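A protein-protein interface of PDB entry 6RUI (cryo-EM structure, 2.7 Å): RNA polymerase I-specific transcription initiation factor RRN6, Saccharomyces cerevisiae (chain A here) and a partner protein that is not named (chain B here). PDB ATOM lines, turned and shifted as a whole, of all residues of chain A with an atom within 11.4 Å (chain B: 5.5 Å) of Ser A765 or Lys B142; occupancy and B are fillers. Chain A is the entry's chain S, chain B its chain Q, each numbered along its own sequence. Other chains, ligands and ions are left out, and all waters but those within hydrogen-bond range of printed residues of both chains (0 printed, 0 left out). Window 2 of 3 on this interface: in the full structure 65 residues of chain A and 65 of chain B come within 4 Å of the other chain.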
ATOM      1  N   SER A 648      18.296  -8.198 -17.103  1.00  0.00           N
ATOM      2  CA  SER A 648      16.831  -8.126 -17.173  1.00  0.00           C
ATOM      3  C   SER A 648      16.331  -7.375 -18.406  1.00  0.00           C
ATOM      4  O   SER A 648      15.290  -6.715 -18.362  1.00  0.00           O
ATOM      5  CB  SER A 648      16.238  -7.511 -15.901  1.00  0.00           C
ATOM      6  OG  SER A 648      16.494  -8.322 -14.769  1.00  0.00           O
ATOM      7  N   ILE A 649      17.069  -7.461 -19.506  1.00  0.00           N
ATOM      8  CA  ILE A 649      16.627  -6.852 -20.751  1.00  0.00           C
ATOM      9  C   ILE A 649      17.063  -7.703 -21.938  1.00  0.00           C
ATOM     10  O   ILE A 649      16.329  -8.589 -22.379  1.00  0.00           O
ATOM     11  CB  ILE A 649      17.150  -5.417 -20.880  1.00  0.00           C
ATOM     12  CG1 ILE A 649      16.406  -4.683 -21.991  1.00  0.00           C
ATOM     13  CG2 ILE A 649      18.639  -5.414 -21.140  1.00  0.00           C
ATOM     14  CD1 ILE A 649      14.940  -4.468 -21.692  1.00  0.00           C
ATOM     15  N   GLN A 757      15.666 -17.258 -16.455  1.00  0.00           N
ATOM     16  CA  GLN A 757      15.344 -15.969 -15.856  1.00  0.00           C
ATOM     17  C   GLN A 757      15.104 -14.887 -16.900  1.00  0.00           C
ATOM     18  O   GLN A 757      14.591 -13.818 -16.559  1.00  0.00           O
ATOM     19  CB  GLN A 757      16.452 -15.506 -14.907  1.00  0.00           C
ATOM     20  CG  GLN A 757      17.733 -15.075 -15.601  1.00  0.00           C
ATOM     21  CD  GLN A 757      18.777 -14.560 -14.629  1.00  0.00           C
ATOM     22  OE1 GLN A 757      18.537 -14.484 -13.424  1.00  0.00           O
ATOM     23  NE2 GLN A 757      19.939 -14.190 -15.150  1.00  0.00           N
ATOM     24  N   ASN A 758      15.470 -15.129 -18.151  1.00  0.00           N
ATOM     25  CA  ASN A 758      15.128 -14.211 -19.217  1.00  0.00           C
ATOM     26  C   ASN A 758      13.833 -14.611 -19.913  1.00  0.00           C
ATOM     27  O   ASN A 758      13.332 -13.855 -20.754  1.00  0.00           O
ATOM     28  CB  ASN A 758      16.292 -14.129 -20.209  1.00  0.00           C
ATOM     29  CG  ASN A 758      16.341 -12.812 -20.935  1.00  0.00           C
ATOM     30  OD1 ASN A 758      15.465 -11.966 -20.762  1.00  0.00           O
ATOM     31  ND2 ASN A 758      17.394 -12.604 -21.714  1.00  0.00           N
ATOM     32  N   GLU A 759      13.284 -15.785 -19.580  1.00  0.00           N
ATOM     33  CA  GLU A 759      11.928 -16.132 -19.993  1.00  0.00           C
ATOM     34  C   GLU A 759      10.900 -15.356 -19.182  1.00  0.00           C
ATOM     35  O   GLU A 759       9.971 -14.761 -19.743  1.00  0.00           O
ATOM     36  CB  GLU A 759      11.680 -17.637 -19.832  1.00  0.00           C
ATOM     37  CG  GLU A 759      12.439 -18.534 -20.792  1.00  0.00           C
ATOM     38  CD  GLU A 759      12.184 -20.011 -20.562  1.00  0.00           C
ATOM     39  OE1 GLU A 759      11.484 -20.350 -19.586  1.00  0.00           O
ATOM     40  OE2 GLU A 759      12.687 -20.838 -21.353  1.00  0.00           O
ATOM     41  N   ILE A 760      11.074 -15.337 -17.857  1.00  0.00           N
ATOM     42  CA  ILE A 760      10.072 -14.795 -16.949  1.00  0.00           C
ATOM     43  C   ILE A 760       9.958 -13.277 -17.044  1.00  0.00           C
ATOM     44  O   ILE A 760       8.919 -12.715 -16.679  1.00  0.00           O
ATOM     45  CB  ILE A 760      10.400 -15.250 -15.512  1.00  0.00           C
ATOM     46  CG1 ILE A 760      11.813 -14.816 -15.130  1.00  0.00           C
ATOM     47  CG2 ILE A 760      10.278 -16.758 -15.373  1.00  0.00           C
ATOM     48  CD1 ILE A 760      12.186 -15.090 -13.695  1.00  0.00           C
ATOM     49  N   SER A 761      10.988 -12.598 -17.556  1.00  0.00           N
ATOM     50  CA  SER A 761      10.980 -11.141 -17.574  1.00  0.00           C
ATOM     51  C   SER A 761      10.114 -10.574 -18.689  1.00  0.00           C
ATOM     52  O   SER A 761       9.584  -9.467 -18.552  1.00  0.00           O
ATOM     53  CB  SER A 761      12.407 -10.609 -17.717  1.00  0.00           C
ATOM     54  OG  SER A 761      13.200 -10.943 -16.593  1.00  0.00           O
ATOM     55  N   ARG A 762       9.952 -11.305 -19.791  1.00  0.00           N
ATOM     56  CA  ARG A 762       9.280 -10.725 -20.946  1.00  0.00           C
ATOM     57  C   ARG A 762       7.765 -10.815 -20.829  1.00  0.00           C
ATOM     58  O   ARG A 762       7.053  -9.897 -21.251  1.00  0.00           O
ATOM     59  CB  ARG A 762       9.775 -11.398 -22.227  1.00  0.00           C
ATOM     60  CG  ARG A 762      11.255 -11.165 -22.550  1.00  0.00           C
ATOM     61  CD  ARG A 762      11.561  -9.710 -22.891  1.00  0.00           C
ATOM     62  NE  ARG A 762      11.946  -8.930 -21.717  1.00  0.00           N
ATOM     63  CZ  ARG A 762      11.975  -7.605 -21.670  1.00  0.00           C
ATOM     64  NH1 ARG A 762      12.333  -6.989 -20.552  1.00  0.00           N
ATOM     65  NH2 ARG A 762      11.641  -6.897 -22.740  1.00  0.00           N
ATOM     66  N   SER A 763       7.259 -11.908 -20.253  1.00  0.00           N
ATOM     67  CA  SER A 763       5.821 -12.063 -20.075  1.00  0.00           C
ATOM     68  C   SER A 763       5.265 -11.106 -19.035  1.00  0.00           C
ATOM     69  O   SER A 763       4.090 -10.734 -19.123  1.00  0.00           O
ATOM     70  CB  SER A 763       5.494 -13.499 -19.685  1.00  0.00           C
ATOM     71  OG  SER A 763       4.102 -13.663 -19.511  1.00  0.00           O
ATOM     72  N   LEU A 764       6.084 -10.708 -18.055  1.00  0.00           N
ATOM     73  CA  LEU A 764       5.706  -9.627 -17.152  1.00  0.00           C
ATOM     74  C   LEU A 764       5.554  -8.311 -17.905  1.00  0.00           C
ATOM     75  O   LEU A 764       4.651  -7.522 -17.605  1.00  0.00           O
ATOM     76  CB  LEU A 764       6.745  -9.484 -16.038  1.00  0.00           C
ATOM     77  CG  LEU A 764       6.823 -10.559 -14.947  1.00  0.00           C
ATOM     78  CD1 LEU A 764       8.041 -10.350 -14.060  1.00  0.00           C
ATOM     79  CD2 LEU A 764       5.554 -10.569 -14.093  1.00  0.00           C
ATOM     80  N   SER A 765       6.412  -8.074 -18.903  1.00  0.00           N
ATOM     81  CA  SER A 765       6.421  -6.805 -19.623  1.00  0.00           C
ATOM     82  C   SER A 765       5.248  -6.669 -20.582  1.00  0.00           C
ATOM     83  O   SER A 765       4.711  -5.569 -20.741  1.00  0.00           O
ATOM     84  CB  SER A 765       7.734  -6.646 -20.384  1.00  0.00           C
ATOM     85  OG  SER A 765       7.743  -5.429 -21.105  1.00  0.00           O
ATOM     86  N   GLY A 766       4.846  -7.754 -21.236  1.00  0.00           N
ATOM     87  CA  GLY A 766       3.624  -7.750 -22.008  1.00  0.00           C
ATOM     88  C   GLY A 766       2.410  -7.762 -21.108  1.00  0.00           C
ATOM     89  O   GLY A 766       2.481  -8.062 -19.904  1.00  0.00           O
ATOM     90  N   PRO A 767       1.251  -7.440 -21.686  1.00  0.00           N
ATOM     91  CA  PRO A 767       0.050  -7.293 -20.859  1.00  0.00           C
ATOM     92  C   PRO A 767      -0.528  -8.636 -20.457  1.00  0.00           C
ATOM     93  O   PRO A 767       0.011  -9.689 -20.815  1.00  0.00           O
ATOM     94  CB  PRO A 767      -0.907  -6.515 -21.772  1.00  0.00           C
ATOM     95  CG  PRO A 767      -0.527  -6.956 -23.134  1.00  0.00           C
ATOM     96  CD  PRO A 767       0.962  -7.215 -23.110  1.00  0.00           C
ATOM     97  N   TYR A 768      -1.639  -8.612 -19.731  1.00  0.00           N
ATOM     98  CA  TYR A 768      -2.332  -9.829 -19.330  1.00  0.00           C
ATOM     99  C   TYR A 768      -3.097 -10.482 -20.478  1.00  0.00           C
ATOM    100  O   TYR A 768      -3.693 -11.545 -20.281  1.00  0.00           O
ATOM    101  CB  TYR A 768      -3.276  -9.539 -18.154  1.00  0.00           C
ATOM    102  CG  TYR A 768      -4.367  -8.526 -18.443  1.00  0.00           C
ATOM    103  CD1 TYR A 768      -4.151  -7.171 -18.239  1.00  0.00           C
ATOM    104  CD2 TYR A 768      -5.624  -8.932 -18.891  1.00  0.00           C
ATOM    105  CE1 TYR A 768      -5.143  -6.244 -18.496  1.00  0.00           C
ATOM    106  CE2 TYR A 768      -6.621  -8.011 -19.151  1.00  0.00           C
ATOM    107  CZ  TYR A 768      -6.376  -6.670 -18.951  1.00  0.00           C
ATOM    108  OH  TYR A 768      -7.367  -5.748 -19.200  1.00  0.00           O
ATOM    109  N   GLN A 769      -3.099  -9.869 -21.660  1.00  0.00           N
ATOM    110  CA  GLN A 769      -3.657 -10.489 -22.849  1.00  0.00           C
ATOM    111  C   GLN A 769      -2.697 -11.497 -23.465  1.00  0.00           C
ATOM    112  O   GLN A 769      -3.140 -12.465 -24.093  1.00  0.00           O
ATOM    113  CB  GLN A 769      -4.009  -9.409 -23.874  1.00  0.00           C
ATOM    114  CG  GLN A 769      -4.983  -9.865 -24.929  1.00  0.00           C
ATOM    115  CD  GLN A 769      -6.341 -10.178 -24.325  1.00  0.00           C
ATOM    116  OE1 GLN A 769      -6.685 -11.340 -24.112  1.00  0.00           O
ATOM    117  NE2 GLN A 769      -7.115  -9.136 -24.048  1.00  0.00           N
ATOM    118  N   ASP A 770      -1.394 -11.309 -23.271  1.00  0.00           N
ATOM    119  CA  ASP A 770      -0.378 -12.213 -23.788  1.00  0.00           C
ATOM    120  C   ASP A 770       0.075 -13.252 -22.768  1.00  0.00           C
ATOM    121  O   ASP A 770       1.044 -13.972 -23.025  1.00  0.00           O
ATOM    122  CB  ASP A 770       0.823 -11.416 -24.293  1.00  0.00           C
ATOM    123  CG  ASP A 770       0.508 -10.627 -25.545  1.00  0.00           C
ATOM    124  OD1 ASP A 770      -0.384 -11.056 -26.304  1.00  0.00           O
ATOM    125  OD2 ASP A 770       1.155  -9.583 -25.776  1.00  0.00           O
ATOM    126  N   ILE A 771      -0.596 -13.335 -21.615  1.00  0.00           N
ATOM    127  CA  ILE A 771      -0.344 -14.425 -20.674  1.00  0.00           C
ATOM    128  C   ILE A 771      -0.837 -15.745 -21.251  1.00  0.00           C
ATOM    129  O   ILE A 771      -0.089 -16.727 -21.337  1.00  0.00           O
ATOM    130  CB  ILE A 771      -1.004 -14.131 -19.314  1.00  0.00           C
ATOM    131  CG1 ILE A 771      -0.339 -12.943 -18.618  1.00  0.00           C
ATOM    132  CG2 ILE A 771      -0.952 -15.353 -18.425  1.00  0.00           C
ATOM    133  CD1 ILE A 771       1.095 -13.193 -18.212  1.00  0.00           C
ATOM    134  N   SER A 773      -1.613 -16.288 -24.283  1.00  0.00           N
ATOM    135  CA  SER A 773      -1.014 -16.514 -25.592  1.00  0.00           C
ATOM    136  C   SER A 773       0.301 -17.278 -25.521  1.00  0.00           C
ATOM    137  O   SER A 773       0.718 -17.841 -26.532  1.00  0.00           O
ATOM    138  CB  SER A 773      -0.790 -15.181 -26.306  1.00  0.00           C
ATOM    139  OG  SER A 773      -0.140 -15.375 -27.545  1.00  0.00           O
ATOM    140  N   SER A 774       0.968 -17.304 -24.367  1.00  0.00           N
ATOM    141  CA  SER A 774       2.282 -17.936 -24.248  1.00  0.00           C
ATOM    142  C   SER A 774       2.175 -19.183 -23.376  1.00  0.00           C
ATOM    143  O   SER A 774       2.366 -19.145 -22.160  1.00  0.00           O
ATOM    144  CB  SER A 774       3.299 -16.953 -23.683  1.00  0.00           C
ATOM    145  OG  SER A 774       4.546 -17.590 -23.481  1.00  0.00           O
ATOM    146  N   LEU B 138       9.513 -14.806 -27.201  1.00  0.00           N
ATOM    147  CA  LEU B 138       8.893 -13.965 -26.183  1.00  0.00           C
ATOM    148  C   LEU B 138       9.107 -12.487 -26.476  1.00  0.00           C
ATOM    149  O   LEU B 138       8.246 -11.657 -26.159  1.00  0.00           O
ATOM    150  CB  LEU B 138       9.419 -14.325 -24.794  1.00  0.00           C
ATOM    151  CG  LEU B 138       8.913 -15.662 -24.241  1.00  0.00           C
ATOM    152  CD1 LEU B 138       9.604 -16.011 -22.942  1.00  0.00           C
ATOM    153  CD2 LEU B 138       7.408 -15.641 -24.062  1.00  0.00           C
ATOM    154  N   LYS B 139      10.239 -12.138 -27.089  1.00  0.00           N
ATOM    155  CA  LYS B 139      10.501 -10.736 -27.396  1.00  0.00           C
ATOM    156  C   LYS B 139       9.681 -10.260 -28.582  1.00  0.00           C
ATOM    157  O   LYS B 139       9.210  -9.117 -28.594  1.00  0.00           O
ATOM    158  CB  LYS B 139      11.976 -10.514 -27.693  1.00  0.00           C
ATOM    159  CG  LYS B 139      12.925 -10.561 -26.529  1.00  0.00           C
ATOM    160  CD  LYS B 139      14.292 -10.164 -27.046  1.00  0.00           C
ATOM    161  CE  LYS B 139      14.837 -11.218 -27.993  1.00  0.00           C
ATOM    162  NZ  LYS B 139      16.162 -10.824 -28.514  1.00  0.00           N
ATOM    163  N   ILE B 140       9.505 -11.119 -29.592  1.00  0.00           N
ATOM    164  CA  ILE B 140       8.923 -10.698 -30.864  1.00  0.00           C
ATOM    165  C   ILE B 140       7.437 -10.382 -30.725  1.00  0.00           C
ATOM    166  O   ILE B 140       6.871  -9.661 -31.557  1.00  0.00           O
ATOM    167  CB  ILE B 140       9.207 -11.782 -31.930  1.00  0.00           C
ATOM    168  CG1 ILE B 140       8.993 -11.259 -33.346  1.00  0.00           C
ATOM    169  CG2 ILE B 140       8.360 -12.996 -31.718  1.00  0.00           C
ATOM    170  CD1 ILE B 140       9.955 -10.212 -33.725  1.00  0.00           C
ATOM    171  N   LEU B 141       6.803 -10.859 -29.655  1.00  0.00           N
ATOM    172  CA  LEU B 141       5.430 -10.485 -29.364  1.00  0.00           C
ATOM    173  C   LEU B 141       5.341  -9.082 -28.777  1.00  0.00           C
ATOM    174  O   LEU B 141       4.310  -8.416 -28.922  1.00  0.00           O
ATOM    175  CB  LEU B 141       4.833 -11.519 -28.415  1.00  0.00           C
ATOM    176  CG  LEU B 141       3.358 -11.458 -28.060  1.00  0.00           C
ATOM    177  CD1 LEU B 141       2.558 -11.574 -29.326  1.00  0.00           C
ATOM    178  CD2 LEU B 141       3.023 -12.594 -27.109  1.00  0.00           C
ATOM    179  N   LYS B 142       6.417  -8.605 -28.144  1.00  0.00           N
ATOM    180  CA  LYS B 142       6.379  -7.309 -27.475  1.00  0.00           C
ATOM    181  C   LYS B 142       6.461  -6.163 -28.474  1.00  0.00           C
ATOM    182  O   LYS B 142       6.026  -5.047 -28.174  1.00  0.00           O
ATOM    183  CB  LYS B 142       7.513  -7.227 -26.448  1.00  0.00           C
ATOM    184  CG  LYS B 142       7.416  -6.114 -25.393  1.00  0.00           C
ATOM    185  CD  LYS B 142       8.203  -4.853 -25.754  1.00  0.00           C
ATOM    186  CE  LYS B 142       8.332  -3.927 -24.554  1.00  0.00           C
ATOM    187  NZ  LYS B 142       7.011  -3.458 -24.056  1.00  0.00           N
ATOM    188  N   THR B 143       7.017  -6.410 -29.659  1.00  0.00           N
ATOM    189  CA  THR B 143       6.989  -5.378 -30.688  1.00  0.00           C
ATOM    190  C   THR B 143       5.574  -5.202 -31.225  1.00  0.00           C
ATOM    191  O   THR B 143       5.172  -4.092 -31.588  1.00  0.00           O
ATOM    192  CB  THR B 143       7.971  -5.739 -31.798  1.00  0.00           C
ATOM    193  OG1 THR B 143       9.231  -6.086 -31.211  1.00  0.00           O
ATOM    194  CG2 THR B 143       8.197  -4.546 -32.715  1.00  0.00           C
ATOM    195  N   ILE B 144       4.797  -6.282 -31.229  1.00  0.00           N
ATOM    196  CA  ILE B 144       3.381  -6.223 -31.562  1.00  0.00           C
ATOM    197  C   ILE B 144       2.571  -5.649 -30.396  1.00  0.00           C
ATOM    198  O   ILE B 144       1.488  -5.084 -30.601  1.00  0.00           O
ATOM    199  CB  ILE B 144       2.942  -7.642 -31.971  1.00  0.00           C
ATOM    200  CG1 ILE B 144       3.814  -8.122 -33.130  1.00  0.00           C
ATOM    201  CG2 ILE B 144       1.493  -7.712 -32.397  1.00  0.00           C
ATOM    202  CD1 ILE B 144       3.696  -7.260 -34.378  1.00  0.00           C
ATOM    203  N   ASN B 145       3.093  -5.760 -29.166  1.00  0.00           N
ATOM    204  CA  ASN B 145       2.435  -5.187 -27.989  1.00  0.00           C
ATOM    205  C   ASN B 145       2.336  -3.671 -28.086  1.00  0.00           C
ATOM    206  O   ASN B 145       1.263  -3.096 -27.874  1.00  0.00           O
ATOM    207  CB  ASN B 145       3.212  -5.572 -26.730  1.00  0.00           C
ATOM    208  CG  ASN B 145       2.526  -5.162 -25.446  1.00  0.00           C
ATOM    209  OD1 ASN B 145       1.358  -4.776 -25.423  1.00  0.00           O
ATOM    210  ND2 ASN B 145       3.286  -5.192 -24.359  1.00  0.00           N
ATOM    211  N   ASP B 146       3.433  -3.010 -28.443  1.00  0.00           N
ATOM    212  CA  ASP B 146       3.482  -1.555 -28.465  1.00  0.00           C
ATOM    213  C   ASP B 146       2.853  -0.972 -29.731  1.00  0.00           C
ATOM    214  O   ASP B 146       2.974   0.233 -29.978  1.00  0.00           O
ATOM    215  CB  ASP B 146       4.936  -1.102 -28.297  1.00  0.00           C
ATOM    216  CG  ASP B 146       5.057   0.269 -27.653  1.00  0.00           C
ATOM    217  OD1 ASP B 146       4.023   0.924 -27.415  1.00  0.00           O
ATOM    218  OD2 ASP B 146       6.195   0.673 -27.336  1.00  0.00           O
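Among the printed residues, merely in contact across the chains: Glu A759 with Leu B138 (3.5 Å), Arg A762 with Leu B138 (3.9 Å), Arg A762 with Lys B139 (3.98 Å), Ser A765 with Lys B142 (3.6 Å), Ser A765 with Asn B145 (3.9 Å), Gly A766 with Asn B145 (3.5 Å), Pro A767 with Asn B145 (3.3 Å), Asp A770 with Leu B141 (3.6 Å) and Ser A774 with Leu B138 (3.5 Å).
Lys B142 touches just one residue of chain A: Ser A765. No residue of chain A comes within 4 Å of Ile B140. Of chain A, only Asp A770 (3.6 Å) comes within 4 Å of Leu B141. No residue of chain A comes within 4 Å of Thr B143. No residue of chain A comes within 4 Å of Ile B144. Of the printed residues of chain B, Ser A774 touches Leu B138 (3.5 Å). Printed residues of chain A within 4 Å of Leu B138: Glu A759, Arg A762 and Ser A774. Printed residues of chain B within 4 Å of Arg A762: Leu B138 (3.9 Å) and Lys B139 (3.98 Å). Of the printed residues of chain B, Pro A767 touches Asn B145. Of the printed residues of chain B, Glu A759 touches Leu B138 (3.5 Å). The nearest residue of chain A that does not touch Lys B142 is Arg A762 (4.8 Å). The nearest printed residue of chain A that does not touch Leu B138 is Asn A758 (4.8 Å).
Of the 19 printed residues of chain A, 7 touch a printed residue of chain B. Hydrophobic or aromatic side chains of chain B within 4 Å of the printed part of chain A: Leu B138 and Leu B141. Among the printed residues, 9 pairs touch across the chains. Among the printed residues, no Asp or Glu carboxylate lies within 4 Å of a Lys or Arg side-chain nitrogen of the other chain.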
